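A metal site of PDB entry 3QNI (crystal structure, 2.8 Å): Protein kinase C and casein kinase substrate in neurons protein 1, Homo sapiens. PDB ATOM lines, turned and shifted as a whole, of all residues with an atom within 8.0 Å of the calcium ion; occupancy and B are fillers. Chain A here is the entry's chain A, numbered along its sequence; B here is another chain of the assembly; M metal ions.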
ATOM      1  N   ARG A  68      16.902  -2.750  15.477  1.00  0.00           N
ATOM      2  CA  ARG A  68      15.917  -1.784  15.017  1.00  0.00           C
ATOM      3  C   ARG A  68      16.636  -0.528  14.563  1.00  0.00           C
ATOM      4  O   ARG A  68      16.349  -0.045  13.486  1.00  0.00           O
ATOM      5  CB  ARG A  68      14.898  -1.432  16.112  1.00  0.00           C
ATOM      6  CG  ARG A  68      13.469  -1.550  15.665  1.00  0.00           C
ATOM      7  CD  ARG A  68      12.471  -0.805  16.519  1.00  0.00           C
ATOM      8  NE  ARG A  68      12.422  -1.258  17.918  1.00  0.00           N
ATOM      9  CZ  ARG A  68      11.974  -2.461  18.330  1.00  0.00           C
ATOM     10  NH1 ARG A  68      12.010  -2.732  19.628  1.00  0.00           N
ATOM     11  NH2 ARG A  68      11.495  -3.368  17.470  1.00  0.00           N
ATOM     12  N   GLN A  69      17.566  -0.022  15.359  1.00  0.00           N
ATOM     13  CA  GLN A  69      18.322   1.165  14.984  1.00  0.00           C
ATOM     14  C   GLN A  69      19.250   0.882  13.786  1.00  0.00           C
ATOM     15  O   GLN A  69      19.174   1.578  12.765  1.00  0.00           O
ATOM     16  CB  GLN A  69      19.113   1.720  16.186  1.00  0.00           C
ATOM     17  CG  GLN A  69      18.337   2.672  17.122  1.00  0.00           C
ATOM     18  CD  GLN A  69      18.319   4.154  16.615  1.00  0.00           C
ATOM     19  OE1 GLN A  69      19.047   5.015  17.163  1.00  0.00           O
ATOM     20  NE2 GLN A  69      17.519   4.446  15.569  1.00  0.00           N
ATOM     21  N   LEU A  70      20.092  -0.153  13.870  1.00  0.00           N
ATOM     22  CA  LEU A  70      21.006  -0.461  12.774  1.00  0.00           C
ATOM     23  C   LEU A  70      20.275  -0.549  11.401  1.00  0.00           C
ATOM     24  O   LEU A  70      20.800  -0.077  10.382  1.00  0.00           O
ATOM     25  CB  LEU A  70      21.794  -1.742  13.072  1.00  0.00           C
ATOM     26  CG  LEU A  70      22.945  -1.565  14.073  1.00  0.00           C
ATOM     27  CD1 LEU A  70      23.581  -2.878  14.500  1.00  0.00           C
ATOM     28  CD2 LEU A  70      24.035  -0.678  13.588  1.00  0.00           C
ATOM     29  N   ILE A  71      19.089  -1.170  11.387  1.00  0.00           N
ATOM     30  CA  ILE A  71      18.306  -1.340  10.168  1.00  0.00           C
ATOM     31  C   ILE A  71      17.727  -0.024   9.694  1.00  0.00           C
ATOM     32  O   ILE A  71      17.642   0.219   8.489  1.00  0.00           O
ATOM     33  CB  ILE A  71      17.153  -2.316  10.371  1.00  0.00           C
ATOM     34  CG1 ILE A  71      17.656  -3.732  10.435  1.00  0.00           C
ATOM     35  CG2 ILE A  71      16.172  -2.264   9.189  1.00  0.00           C
ATOM     36  CD1 ILE A  71      16.532  -4.698  10.699  1.00  0.00           C
ATOM     37  N   GLU A  72      17.300   0.806  10.634  1.00  0.00           N
ATOM     38  CA  GLU A  72      16.773   2.124  10.319  1.00  0.00           C
ATOM     39  C   GLU A  72      17.839   3.045   9.749  1.00  0.00           C
ATOM     40  O   GLU A  72      17.678   3.604   8.658  1.00  0.00           O
ATOM     41  CB  GLU A  72      16.188   2.728  11.594  1.00  0.00           C
ATOM     42  CG  GLU A  72      16.507   4.180  11.829  1.00  0.00           C
ATOM     43  CD  GLU A  72      15.356   5.082  11.537  1.00  0.00           C
ATOM     44  OE1 GLU A  72      15.476   6.328  11.799  1.00  0.00           O
ATOM     45  OE2 GLU A  72      14.322   4.535  11.059  1.00  0.00           O
ATOM     46  N   LYS A  73      18.942   3.156  10.467  1.00  0.00           N
ATOM     47  CA  LYS A  73      20.046   4.005  10.078  1.00  0.00           C
ATOM     48  C   LYS A  73      20.814   3.365   8.929  1.00  0.00           C
ATOM     49  O   LYS A  73      21.703   3.985   8.333  1.00  0.00           O
ATOM     50  CB  LYS A  73      20.987   4.227  11.248  1.00  0.00           C
ATOM     51  CG  LYS A  73      20.479   5.178  12.273  1.00  0.00           C
ATOM     52  CD  LYS A  73      21.558   5.428  13.366  1.00  0.00           C
ATOM     53  CE  LYS A  73      21.179   6.641  14.265  1.00  0.00           C
ATOM     54  NZ  LYS A  73      21.122   7.939  13.470  1.00  0.00           N
ATOM     55  N   GLY A  74      20.492   2.115   8.627  1.00  0.00           N
ATOM     56  CA  GLY A  74      21.196   1.423   7.573  1.00  0.00           C
ATOM     57  C   GLY A  74      20.566   1.855   6.295  1.00  0.00           C
ATOM     58  O   GLY A  74      19.618   2.612   6.325  1.00  0.00           O
ATOM     59  N   PRO A  75      21.112   1.382   5.166  1.00  0.00           N
ATOM     60  CA  PRO A  75      20.601   1.628   3.830  1.00  0.00           C
ATOM     61  C   PRO A  75      19.518   0.682   3.291  1.00  0.00           C
ATOM     62  O   PRO A  75      19.187   0.785   2.115  1.00  0.00           O
ATOM     63  CB  PRO A  75      21.855   1.529   2.969  1.00  0.00           C
ATOM     64  CG  PRO A  75      22.735   0.673   3.700  1.00  0.00           C
ATOM     65  CD  PRO A  75      22.513   0.943   5.126  1.00  0.00           C
ATOM     66  N   GLN A  76      18.948  -0.204   4.086  1.00  0.00           N
ATOM     67  CA  GLN A  76      17.861  -1.052   3.561  1.00  0.00           C
ATOM     68  C   GLN A  76      16.500  -0.326   3.690  1.00  0.00           C
ATOM     69  O   GLN A  76      16.152   0.204   4.739  1.00  0.00           O
ATOM     70  CB  GLN A  76      17.869  -2.392   4.274  1.00  0.00           C
ATOM     71  CG  GLN A  76      16.685  -3.302   3.988  1.00  0.00           C
ATOM     72  CD  GLN A  76      16.550  -3.704   2.507  1.00  0.00           C
ATOM     73  OE1 GLN A  76      17.222  -4.636   2.027  1.00  0.00           O
ATOM     74  NE2 GLN A  76      15.647  -3.002   1.786  1.00  0.00           N
ATOM     75  N   TYR A  77      15.733  -0.315   2.603  1.00  0.00           N
ATOM     76  CA  TYR A  77      14.523   0.511   2.469  1.00  0.00           C
ATOM     77  C   TYR A  77      13.336  -0.404   2.089  1.00  0.00           C
ATOM     78  O   TYR A  77      13.511  -1.612   1.890  1.00  0.00           O
ATOM     79  CB  TYR A  77      14.781   1.547   1.368  1.00  0.00           C
ATOM     80  CG  TYR A  77      15.130   0.899   0.020  1.00  0.00           C
ATOM     81  CD1 TYR A  77      16.468   0.598  -0.324  1.00  0.00           C
ATOM     82  CD2 TYR A  77      14.137   0.529  -0.892  1.00  0.00           C
ATOM     83  CE1 TYR A  77      16.779  -0.031  -1.526  1.00  0.00           C
ATOM     84  CE2 TYR A  77      14.447  -0.116  -2.098  1.00  0.00           C
ATOM     85  CZ  TYR A  77      15.761  -0.382  -2.409  1.00  0.00           C
ATOM     86  OH  TYR A  77      16.043  -1.006  -3.598  1.00  0.00           O
ATOM     87  N   GLY A  78      12.126   0.146   2.016  1.00  0.00           N
ATOM     88  CA  GLY A  78      10.995  -0.553   1.391  1.00  0.00           C
ATOM     89  C   GLY A  78      10.436  -1.692   2.216  1.00  0.00           C
ATOM     90  O   GLY A  78      10.668  -1.726   3.417  1.00  0.00           O
ATOM     91  N   GLU A  81      12.870  -3.680   4.294  1.00  0.00           N
ATOM     92  CA  GLU A  81      13.241  -3.095   5.556  1.00  0.00           C
ATOM     93  C   GLU A  81      12.252  -3.544   6.590  1.00  0.00           C
ATOM     94  O   GLU A  81      12.649  -4.025   7.644  1.00  0.00           O
ATOM     95  CB  GLU A  81      13.248  -1.585   5.506  1.00  0.00           C
ATOM     96  CG  GLU A  81      14.244  -0.930   6.469  1.00  0.00           C
ATOM     97  CD  GLU A  81      14.089   0.577   6.519  1.00  0.00           C
ATOM     98  OE1 GLU A  81      14.972   1.283   7.079  1.00  0.00           O
ATOM     99  OE2 GLU A  81      13.059   1.063   5.987  1.00  0.00           O
ATOM    100  N   TRP A  84      12.429  -7.478   7.430  1.00  0.00           N
ATOM    101  CA  TRP A  84      13.548  -7.620   8.324  1.00  0.00           C
ATOM    102  C   TRP A  84      13.236  -7.095   9.724  1.00  0.00           C
ATOM    103  O   TRP A  84      13.344  -7.834  10.691  1.00  0.00           O
ATOM    104  CB  TRP A  84      14.720  -6.892   7.731  1.00  0.00           C
ATOM    105  CG  TRP A  84      15.954  -7.204   8.423  1.00  0.00           C
ATOM    106  CD1 TRP A  84      16.112  -8.074   9.451  1.00  0.00           C
ATOM    107  CD2 TRP A  84      17.252  -6.682   8.118  1.00  0.00           C
ATOM    108  NE1 TRP A  84      17.435  -8.103   9.827  1.00  0.00           N
ATOM    109  CE2 TRP A  84      18.153  -7.257   9.031  1.00  0.00           C
ATOM    110  CE3 TRP A  84      17.734  -5.766   7.178  1.00  0.00           C
ATOM    111  CZ2 TRP A  84      19.501  -6.957   9.042  1.00  0.00           C
ATOM    112  CZ3 TRP A  84      19.061  -5.470   7.181  1.00  0.00           C
ATOM    113  CH2 TRP A  84      19.939  -6.053   8.111  1.00  0.00           C
ATOM    114  N   LEU B  38      24.896  -4.973   3.298  1.00  0.00           N
ATOM    115  CA  LEU B  38      23.691  -5.437   3.928  1.00  0.00           C
ATOM    116  C   LEU B  38      23.702  -6.952   4.181  1.00  0.00           C
ATOM    117  O   LEU B  38      22.983  -7.457   5.072  1.00  0.00           O
ATOM    118  CB  LEU B  38      22.461  -4.973   3.148  1.00  0.00           C
ATOM    119  CG  LEU B  38      22.181  -3.494   3.394  1.00  0.00           C
ATOM    120  CD1 LEU B  38      21.066  -2.925   2.540  1.00  0.00           C
ATOM    121  CD2 LEU B  38      21.843  -3.322   4.858  1.00  0.00           C
HETATM  122 CA    CA M   1      17.125   1.899   6.467  1.00  0.00          CA
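Of the 14 residues printed, 5 come within 4 Å of the calcium ion. Along chain A the residues within 4 Å of the calcium ion span positions 71 to 81. The nearest printed residue that does not touch the calcium ion is Pro 75 (4.2 Å).
The calcium ion is bound by the side-chain carboxylate (OE1) of Glu 81 (2.3 Å), the backbone carbonyl oxygen (O) of Gly 74 (2.6 Å), the backbone carbonyl oxygen (O) of Gln 76 (2.6 Å), the backbone carbonyl oxygen (O) of Ile 71 (2.7 Å) and the backbone carbonyl oxygen (O) of Glu 72 (2.8 Å). The calcium ion has five donor atoms within binding distance.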
